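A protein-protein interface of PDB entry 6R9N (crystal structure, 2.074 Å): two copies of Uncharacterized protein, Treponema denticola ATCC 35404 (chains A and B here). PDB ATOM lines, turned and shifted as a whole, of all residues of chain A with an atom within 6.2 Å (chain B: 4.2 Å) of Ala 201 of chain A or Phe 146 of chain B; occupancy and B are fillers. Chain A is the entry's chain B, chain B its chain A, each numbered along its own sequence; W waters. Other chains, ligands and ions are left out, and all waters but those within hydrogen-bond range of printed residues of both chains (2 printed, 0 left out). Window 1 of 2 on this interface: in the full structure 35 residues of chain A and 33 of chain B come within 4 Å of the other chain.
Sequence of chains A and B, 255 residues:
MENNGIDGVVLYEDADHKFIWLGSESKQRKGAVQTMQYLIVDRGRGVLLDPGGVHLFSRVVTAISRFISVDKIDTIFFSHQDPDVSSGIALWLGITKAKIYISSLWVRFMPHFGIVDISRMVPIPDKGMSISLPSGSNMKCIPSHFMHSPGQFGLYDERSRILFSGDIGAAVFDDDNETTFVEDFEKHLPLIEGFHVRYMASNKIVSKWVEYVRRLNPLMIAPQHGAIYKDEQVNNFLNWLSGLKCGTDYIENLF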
ATOM      1  N   PHE A 146       2.454   0.600   2.898  1.00  0.00           N
ATOM      2  CA  PHE A 146       3.330   1.175   1.869  1.00  0.00           C
ATOM      3  C   PHE A 146       3.325   2.694   1.875  1.00  0.00           C
ATOM      4  O   PHE A 146       3.629   3.334   0.863  1.00  0.00           O
ATOM      5  CB  PHE A 146       2.981   0.621   0.485  1.00  0.00           C
ATOM      6  CG  PHE A 146       3.227  -0.855   0.390  1.00  0.00           C
ATOM      7  CD1 PHE A 146       4.526  -1.341   0.366  1.00  0.00           C
ATOM      8  CD2 PHE A 146       2.170  -1.761   0.437  1.00  0.00           C
ATOM      9  CE1 PHE A 146       4.774  -2.707   0.323  1.00  0.00           C
ATOM     10  CE2 PHE A 146       2.411  -3.133   0.390  1.00  0.00           C
ATOM     11  CZ  PHE A 146       3.718  -3.609   0.344  1.00  0.00           C
ATOM     12  N   MET A 147       3.029   3.285   3.033  1.00  0.00           N
ATOM     13  CA  MET A 147       3.050   4.725   3.173  1.00  0.00           C
ATOM     14  C   MET A 147       3.710   5.150   4.484  1.00  0.00           C
ATOM     15  O   MET A 147       3.137   5.910   5.268  1.00  0.00           O
ATOM     16  CB  MET A 147       1.621   5.275   3.082  1.00  0.00           C
ATOM     17  CG  MET A 147       0.983   5.134   1.686  1.00  0.00           C
ATOM     18  SD  MET A 147      -0.806   5.452   1.618  1.00  0.00           S
ATOM     19  CE  MET A 147      -0.902   7.123   2.254  1.00  0.00           C
ATOM     20  N   HIS A 148       4.959   4.728   4.724  1.00  0.00           N
ATOM     21  CA  HIS A 148       5.851   4.010   3.806  1.00  0.00           C
ATOM     22  C   HIS A 148       5.946   2.515   4.101  1.00  0.00           C
ATOM     23  O   HIS A 148       6.258   1.707   3.222  1.00  0.00           O
ATOM     24  CB  HIS A 148       7.258   4.590   3.909  1.00  0.00           C
ATOM     25  CG  HIS A 148       7.800   4.538   5.305  1.00  0.00           C
ATOM     26  ND1 HIS A 148       8.434   3.427   5.821  1.00  0.00           N
ATOM     27  CD2 HIS A 148       7.724   5.432   6.318  1.00  0.00           C
ATOM     28  CE1 HIS A 148       8.765   3.658   7.079  1.00  0.00           C
ATOM     29  NE2 HIS A 148       8.330   4.863   7.412  1.00  0.00           N
ATOM     30  N   HIS A 196       6.652  13.306   1.586  1.00  0.00           N
ATOM     31  CA  HIS A 196       5.637  12.458   0.962  1.00  0.00           C
ATOM     32  C   HIS A 196       6.031  12.041  -0.451  1.00  0.00           C
ATOM     33  O   HIS A 196       5.786  10.902  -0.851  1.00  0.00           O
ATOM     34  CB  HIS A 196       4.294  13.187   0.959  1.00  0.00           C
ATOM     35  CG  HIS A 196       3.681  13.299   2.319  1.00  0.00           C
ATOM     36  ND1 HIS A 196       4.074  14.254   3.235  1.00  0.00           N
ATOM     37  CD2 HIS A 196       2.738  12.548   2.936  1.00  0.00           C
ATOM     38  CE1 HIS A 196       3.392  14.091   4.356  1.00  0.00           C
ATOM     39  NE2 HIS A 196       2.567  13.071   4.198  1.00  0.00           N
ATOM     40  N   VAL A 197       6.648  12.940  -1.225  1.00  0.00           N
ATOM     41  CA  VAL A 197       7.060  12.575  -2.579  1.00  0.00           C
ATOM     42  C   VAL A 197       8.030  11.391  -2.547  1.00  0.00           C
ATOM     43  O   VAL A 197       7.953  10.488  -3.388  1.00  0.00           O
ATOM     44  CB  VAL A 197       7.667  13.796  -3.305  1.00  0.00           C
ATOM     45  CG1 VAL A 197       8.379  13.373  -4.586  1.00  0.00           C
ATOM     46  CG2 VAL A 197       6.579  14.839  -3.629  1.00  0.00           C
ATOM     47  N   ARG A 198       8.931  11.351  -1.557  1.00  0.00           N
ATOM     48  CA  ARG A 198       9.993  10.348  -1.544  1.00  0.00           C
ATOM     49  C   ARG A 198       9.652   9.086  -0.740  1.00  0.00           C
ATOM     50  O   ARG A 198      10.099   7.982  -1.107  1.00  0.00           O
ATOM     51  CB  ARG A 198      11.283  10.979  -1.012  1.00  0.00           C
ATOM     52  CG  ARG A 198      12.488  10.038  -0.970  1.00  0.00           C
ATOM     53  CD  ARG A 198      12.843   9.466  -2.338  1.00  0.00           C
ATOM     54  NE  ARG A 198      13.909   8.485  -2.200  1.00  0.00           N
ATOM     55  CZ  ARG A 198      13.734   7.216  -1.835  1.00  0.00           C
ATOM     56  NH1 ARG A 198      12.503   6.734  -1.592  1.00  0.00           N
ATOM     57  NH2 ARG A 198      14.797   6.420  -1.715  1.00  0.00           N
ATOM     58  N   TYR A 199       8.879   9.200   0.342  1.00  0.00           N
ATOM     59  CA  TYR A 199       8.676   8.055   1.225  1.00  0.00           C
ATOM     60  C   TYR A 199       7.395   7.269   0.940  1.00  0.00           C
ATOM     61  O   TYR A 199       7.363   6.058   1.184  1.00  0.00           O
ATOM     62  CB  TYR A 199       8.644   8.507   2.695  1.00  0.00           C
ATOM     63  CG  TYR A 199       9.957   8.974   3.306  1.00  0.00           C
ATOM     64  CD1 TYR A 199      10.562  10.151   2.888  1.00  0.00           C
ATOM     65  CD2 TYR A 199      10.572   8.252   4.343  1.00  0.00           C
ATOM     66  CE1 TYR A 199      11.733  10.601   3.458  1.00  0.00           C
ATOM     67  CE2 TYR A 199      11.762   8.695   4.921  1.00  0.00           C
ATOM     68  CZ  TYR A 199      12.329   9.883   4.470  1.00  0.00           C
ATOM     69  OH  TYR A 199      13.503  10.365   5.006  1.00  0.00           O
ATOM     70  N   MET A 200       6.342   7.905   0.439  1.00  0.00           N
ATOM     71  CA  MET A 200       5.148   7.173   0.019  1.00  0.00           C
ATOM     72  C   MET A 200       5.418   6.441  -1.286  1.00  0.00           C
ATOM     73  O   MET A 200       6.058   6.984  -2.185  1.00  0.00           O
ATOM     74  CB  MET A 200       3.973   8.131  -0.162  1.00  0.00           C
ATOM     75  CG  MET A 200       3.847   9.135   0.960  1.00  0.00           C
ATOM     76  SD  MET A 200       3.159   8.373   2.432  1.00  0.00           S
ATOM     77  CE  MET A 200       4.336   8.889   3.699  1.00  0.00           C
ATOM     78  N   ALA A 201       4.898   5.209  -1.400  1.00  0.00           N
ATOM     79  CA  ALA A 201       5.387   4.277  -2.422  1.00  0.00           C
ATOM     80  C   ALA A 201       4.926   4.627  -3.837  1.00  0.00           C
ATOM     81  O   ALA A 201       5.680   4.411  -4.795  1.00  0.00           O
ATOM     82  CB  ALA A 201       4.965   2.851  -2.078  1.00  0.00           C
ATOM     83  N   SER A 202       3.713   5.165  -4.001  1.00  0.00           N
ATOM     84  CA  SER A 202       3.135   5.426  -5.327  1.00  0.00           C
ATOM     85  C   SER A 202       1.848   6.231  -5.186  1.00  0.00           C
ATOM     86  O   SER A 202       1.215   6.240  -4.123  1.00  0.00           O
ATOM     87  CB  SER A 202       2.827   4.121  -6.077  1.00  0.00           C
ATOM     88  OG  SER A 202       1.806   3.409  -5.378  1.00  0.00           O
ATOM     89  N   ASN A 203       1.457   6.906  -6.280  1.00  0.00           N
ATOM     90  CA  ASN A 203       0.146   7.544  -6.280  1.00  0.00           C
ATOM     91  C   ASN A 203      -0.967   6.510  -6.187  1.00  0.00           C
ATOM     92  O   ASN A 203      -2.018   6.787  -5.604  1.00  0.00           O
ATOM     93  CB  ASN A 203      -0.060   8.415  -7.518  1.00  0.00           C
ATOM     94  CG  ASN A 203      -1.396   9.171  -7.482  1.00  0.00           C
ATOM     95  OD1 ASN A 203      -2.345   8.791  -8.157  1.00  0.00           O
ATOM     96  ND2 ASN A 203      -1.477  10.209  -6.654  1.00  0.00           N
ATOM     97  N   ILE A 205      -1.139   3.869  -4.294  1.00  0.00           N
ATOM     98  CA  ILE A 205      -1.480   3.516  -2.922  1.00  0.00           C
ATOM     99  C   ILE A 205      -2.061   4.714  -2.164  1.00  0.00           C
ATOM    100  O   ILE A 205      -3.048   4.561  -1.435  1.00  0.00           O
ATOM    101  CB  ILE A 205      -0.267   2.867  -2.204  1.00  0.00           C
ATOM    102  CG1 ILE A 205      -0.710   2.194  -0.906  1.00  0.00           C
ATOM    103  CG2 ILE A 205       0.833   3.857  -1.901  1.00  0.00           C
ATOM    104  CD1 ILE A 205      -1.746   1.110  -1.083  1.00  0.00           C
ATOM    105  N   VAL A 206      -1.520   5.928  -2.356  1.00  0.00           N
ATOM    106  CA  VAL A 206      -1.961   7.050  -1.524  1.00  0.00           C
ATOM    107  C   VAL A 206      -3.378   7.489  -1.876  1.00  0.00           C
ATOM    108  O   VAL A 206      -4.133   7.944  -1.001  1.00  0.00           O
ATOM    109  CB  VAL A 206      -0.979   8.241  -1.578  1.00  0.00           C
ATOM    110  CG1 VAL A 206       0.438   7.798  -1.175  1.00  0.00           C
ATOM    111  CG2 VAL A 206      -1.004   8.965  -2.927  1.00  0.00           C
ATOM    112  N   CYS A 246       4.496  10.130  -6.450  1.00  0.00           N
ATOM    113  CA  CYS A 246       5.428   9.849  -5.362  1.00  0.00           C
ATOM    114  C   CYS A 246       6.079   8.491  -5.563  1.00  0.00           C
ATOM    115  O   CYS A 246       5.561   7.635  -6.288  1.00  0.00           O
ATOM    116  CB  CYS A 246       4.770   9.925  -3.999  1.00  0.00           C
ATOM    117  SG  CYS A 246       3.320   8.906  -3.938  1.00  0.00           S
ATOM    118  N   GLY A 247       7.249   8.323  -4.937  1.00  0.00           N
ATOM    119  CA  GLY A 247       7.824   7.002  -4.729  1.00  0.00           C
ATOM    120  C   GLY A 247       8.238   6.386  -6.043  1.00  0.00           C
ATOM    121  O   GLY A 247       9.017   7.001  -6.783  1.00  0.00           O
ATOM    122  N   THR A 248       7.713   5.203  -6.372  1.00  0.00           N
ATOM    123  CA  THR A 248       8.131   4.580  -7.628  1.00  0.00           C
ATOM    124  C   THR A 248       7.579   5.292  -8.854  1.00  0.00           C
ATOM    125  O   THR A 248       8.008   4.972  -9.969  1.00  0.00           O
ATOM    126  CB  THR A 248       7.724   3.098  -7.704  1.00  0.00           C
ATOM    127  OG1 THR A 248       6.299   2.979  -7.672  1.00  0.00           O
ATOM    128  CG2 THR A 248       8.342   2.295  -6.565  1.00  0.00           C
ATOM    129  N   ASP A 249       6.640   6.238  -8.679  1.00  0.00           N
ATOM    130  CA  ASP A 249       6.233   7.073  -9.800  1.00  0.00           C
ATOM    131  C   ASP A 249       7.437   7.810 -10.391  1.00  0.00           C
ATOM    132  O   ASP A 249       7.414   8.186 -11.565  1.00  0.00           O
ATOM    133  CB  ASP A 249       5.164   8.090  -9.366  1.00  0.00           C
ATOM    134  CG  ASP A 249       3.854   7.450  -8.886  1.00  0.00           C
ATOM    135  OD1 ASP A 249       3.587   6.269  -9.194  1.00  0.00           O
ATOM    136  OD2 ASP A 249       3.083   8.154  -8.192  1.00  0.00           O
ATOM    137  N   LEU A 254      15.409   6.497  -8.573  1.00  0.00           N
ATOM    138  CA  LEU A 254      15.748   5.454  -7.603  1.00  0.00           C
ATOM    139  C   LEU A 254      16.848   4.512  -8.080  1.00  0.00           C
ATOM    140  O   LEU A 254      17.254   3.628  -7.322  1.00  0.00           O
ATOM    141  CB  LEU A 254      14.503   4.629  -7.248  1.00  0.00           C
ATOM    142  CG  LEU A 254      13.241   5.365  -6.773  1.00  0.00           C
ATOM    143  CD1 LEU A 254      12.105   4.373  -6.534  1.00  0.00           C
ATOM    144  CD2 LEU A 254      13.487   6.190  -5.503  1.00  0.00           C
ATOM    145  N   SER B 144      17.962  -0.282  -3.578  1.00  0.00           N
ATOM    146  CA  SER B 144      17.008  -1.375  -3.381  1.00  0.00           C
ATOM    147  C   SER B 144      15.753  -0.842  -2.738  1.00  0.00           C
ATOM    148  O   SER B 144      15.170  -1.472  -1.848  1.00  0.00           O
ATOM    149  CB  SER B 144      17.617  -2.490  -2.529  1.00  0.00           C
ATOM    150  OG  SER B 144      18.836  -2.940  -3.095  1.00  0.00           O
ATOM    151  N   HIS B 145      15.326   0.334  -3.184  1.00  0.00           N
ATOM    152  CA  HIS B 145      14.297   1.081  -2.489  1.00  0.00           C
ATOM    153  C   HIS B 145      12.928   0.427  -2.663  1.00  0.00           C
ATOM    154  O   HIS B 145      12.637  -0.217  -3.677  1.00  0.00           O
ATOM    155  CB  HIS B 145      14.292   2.530  -2.989  1.00  0.00           C
ATOM    156  CG  HIS B 145      15.631   3.191  -2.893  1.00  0.00           C
ATOM    157  ND1 HIS B 145      16.290   3.366  -1.692  1.00  0.00           N
ATOM    158  CD2 HIS B 145      16.445   3.702  -3.848  1.00  0.00           C
ATOM    159  CE1 HIS B 145      17.448   3.965  -1.913  1.00  0.00           C
ATOM    160  NE2 HIS B 145      17.568   4.177  -3.214  1.00  0.00           N
ATOM    161  N   PHE B 146      12.094   0.573  -1.639  1.00  0.00           N
ATOM    162  CA  PHE B 146      10.726   0.052  -1.655  1.00  0.00           C
ATOM    163  C   PHE B 146      10.678  -1.469  -1.762  1.00  0.00           C
ATOM    164  O   PHE B 146       9.670  -2.037  -2.217  1.00  0.00           O
ATOM    165  CB  PHE B 146       9.901   0.698  -2.773  1.00  0.00           C
ATOM    166  CG  PHE B 146       9.687   2.152  -2.564  1.00  0.00           C
ATOM    167  CD1 PHE B 146       8.812   2.593  -1.588  1.00  0.00           C
ATOM    168  CD2 PHE B 146      10.399   3.082  -3.293  1.00  0.00           C
ATOM    169  CE1 PHE B 146       8.630   3.949  -1.366  1.00  0.00           C
ATOM    170  CE2 PHE B 146      10.211   4.452  -3.075  1.00  0.00           C
ATOM    171  CZ  PHE B 146       9.331   4.874  -2.120  1.00  0.00           C
ATOM    172  N   MET B 147      11.735  -2.148  -1.297  1.00  0.00           N
ATOM    173  CA  MET B 147      11.755  -3.606  -1.265  1.00  0.00           C
ATOM    174  C   MET B 147      12.325  -4.134   0.054  1.00  0.00           C
ATOM    175  O   MET B 147      13.307  -4.871   0.069  1.00  0.00           O
ATOM    176  CB  MET B 147      12.572  -4.156  -2.436  1.00  0.00           C
ATOM    177  CG  MET B 147      11.931  -3.943  -3.808  1.00  0.00           C
ATOM    178  SD  MET B 147      13.061  -4.141  -5.238  1.00  0.00           S
ATOM    179  CE  MET B 147      13.586  -5.851  -5.076  1.00  0.00           C
ATOM    180  N   HIS B 148      11.736  -3.769   1.200  1.00  0.00           N
ATOM    181  CA  HIS B 148      10.491  -3.006   1.358  1.00  0.00           C
ATOM    182  C   HIS B 148      10.688  -1.526   1.675  1.00  0.00           C
ATOM    183  O   HIS B 148       9.820  -0.694   1.380  1.00  0.00           O
ATOM    184  CB  HIS B 148       9.673  -3.605   2.501  1.00  0.00           C
ATOM    185  CG  HIS B 148      10.425  -3.666   3.799  1.00  0.00           C
ATOM    186  ND1 HIS B 148      10.368  -2.669   4.749  1.00  0.00           N
ATOM    187  CD2 HIS B 148      11.278  -4.596   4.286  1.00  0.00           C
ATOM    188  CE1 HIS B 148      11.128  -2.995   5.776  1.00  0.00           C
ATOM    189  NE2 HIS B 148      11.699  -4.160   5.516  1.00  0.00           N
ATOM    190  N   SER B 149      11.816  -1.191   2.286  1.00  0.00           N
ATOM    191  CA  SER B 149      11.921   0.154   2.862  1.00  0.00           C
ATOM    192  C   SER B 149      12.169   1.190   1.764  1.00  0.00           C
ATOM    193  O   SER B 149      12.895   0.906   0.799  1.00  0.00           O
ATOM    194  CB  SER B 149      13.070   0.203   3.883  1.00  0.00           C
ATOM    195  OG  SER B 149      13.474   1.533   4.164  1.00  0.00           O
ATOM    196  N   PRO B 150      11.607   2.402   1.906  1.00  0.00           N
ATOM    197  CA  PRO B 150      11.797   3.431   0.869  1.00  0.00           C
ATOM    198  C   PRO B 150      13.242   3.873   0.707  1.00  0.00           C
ATOM    199  O   PRO B 150      13.585   4.423  -0.347  1.00  0.00           O
ATOM    200  CB  PRO B 150      10.918   4.601   1.341  1.00  0.00           C
ATOM    201  CG  PRO B 150      10.718   4.381   2.809  1.00  0.00           C
ATOM    202  CD  PRO B 150      10.766   2.881   3.024  1.00  0.00           C
ATOM    203  N   ALA B 201       7.091  -3.996  -2.728  1.00  0.00           N
ATOM    204  CA  ALA B 201       6.009  -3.033  -2.972  1.00  0.00           C
ATOM    205  C   ALA B 201       5.230  -3.299  -4.259  1.00  0.00           C
ATOM    206  O   ALA B 201       4.024  -3.018  -4.302  1.00  0.00           O
ATOM    207  CB  ALA B 201       6.528  -1.597  -3.012  1.00  0.00           C
ATOM    208  N   ILE B 205       8.758  -2.221  -9.195  1.00  0.00           N
ATOM    209  CA  ILE B 205      10.042  -1.961  -8.545  1.00  0.00           C
ATOM    210  C   ILE B 205      10.901  -3.219  -8.566  1.00  0.00           C
ATOM    211  O   ILE B 205      12.114  -3.163  -8.818  1.00  0.00           O
ATOM    212  CB  ILE B 205       9.847  -1.418  -7.115  1.00  0.00           C
ATOM    213  CG1 ILE B 205      11.169  -0.884  -6.583  1.00  0.00           C
ATOM    214  CG2 ILE B 205       9.307  -2.487  -6.174  1.00  0.00           C
ATOM    215  CD1 ILE B 205      11.760   0.248  -7.454  1.00  0.00           C
HETATM  216  O   HOH W   1       7.228   0.458   0.739  1.00  0.00           O
HETATM  217  O   HOH W   2      15.953   1.236  -5.729  1.00  0.00           O
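Phe 146 of chain A touches Ala 201 of chain B, and with the chains exchanged Ala 201 of chain A touches Phe 146 of chain B.
Of the 13 pairs that touch across the chains among the printed residues, 2 have their exchanged pair printed and touching as well.
O of Val 197 of chain A is in hydrogen-bond range of N of Gly 247 of chain A (2.8 Å).
N of Ala 201 of chain B lies close to O of Phe 146 of chain B (3.3 Å).
N of Ala 201 of chain A lies within hydrogen-bond range of O of Phe 146 of chain A (3.2 Å).
O of Met 200 of chain A sits close to N of Gly 247 of chain A (3.3 Å).
The side-chain sulfur (SG) of Cys 246 of chain A sits close to the backbone carbonyl oxygen (O) of Met 200 of chain A (3.8 Å).
A ring nitrogen (ND1) of His 145 of chain B is in hydrogen-bond range of the backbone carbonyl oxygen of Pro 150 of chain B (3.2 Å).
Of the printed residues of chain B, Phe 146 of chain A touches Ala 201 (3.5 Å).
Of the printed residues of chain B, His 148 of chain A touches Pro 150.
Ala 201 of chain A touches just one residue of chain B: Phe 146 (3.4 Å).
Of the printed residues of chain B, Gly 247 of chain A touches Phe 146 (3.7 Å).
Of the printed residues of chain B, Leu 254 of chain A touches His 145 (3.6 Å) and Phe 146 (3.9 Å).
Printed residues of chain A within 4 Å of His 145 of chain B: Arg 198 and Leu 254.
Phe 146 of chain B touches seven residues of chain A.
Met 147 of chain B touches none of the printed residues of chain A.
The nearest printed residue of chain A that does not touch Phe 146 of chain B is His 148 of chain A (5.5 Å).
The nearest printed residue of chain B that does not touch Leu 254 of chain A is Ile 205 of chain B (4.2 Å).
Water W2 lies within hydrogen-bond range of N of His 145 of chain B (2.8 Å), O of Leu 254 of chain A (3.2 Å) and N of Ser 144 of chain B (3.3 Å).
Water W1 lies within hydrogen-bond range of O of His 148 of chain B (2.9 Å) and O of His 148 of chain A (2.9 Å).
O of Pro 150 of chain B is in hydrogen-bond range of NH2 of Arg 198 of chain A.
A ring nitrogen (ND1) of His 145 of chain B sits at hydrogen-bond distance from the guanidinium group (NH2) of Arg 198 of chain A (3.4 Å).
Of the 18 printed residues of chain A, 9 touch a printed residue of chain B.
Along chain A the printed residues that touch a printed residue of chain B span positions 146 to 254.
Printed residues of chain B that touch a printed residue of chain A: His 145, Phe 146, Pro 150 and Ala 201.
Hydrophobic or aromatic side chains of chain B that line the printed part of chain A: His 145, Phe 146, Pro 150 and Ala 201.
Along chain B the printed residues that touch a printed residue of chain A span positions 145 to 201.
Phe 146 of chain A touches Ala 201 of chain B (CE1 to CA, 3.5 Å).
His 148 of chain A touches Pro 150 of chain B.
CZ of Phe 146 of chain B touches O of Arg 198 of chain A, 3.4 Å away.
CE1 of Phe 146 of chain B touches O of Tyr 199 of chain A, at 3.5 Å.
Pro 150 of chain B touches Tyr 199 of chain A.
CA of Ala 201 of chain A touches CE1 of Phe 146 of chain B (3.4 Å).
Gly 247 of chain A touches Phe 146 of chain B (CA to CZ, 3.7 Å).
CD2 of Phe 146 of chain B touches CG2 of Thr 248 of chain A (3.9 Å).
O of Leu 254 of chain A touches CD2 of His 145 of chain B (3.6 Å).
CD2 of Phe 146 of chain B touches CD1 of Leu 254 of chain A, at 3.9 Å.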
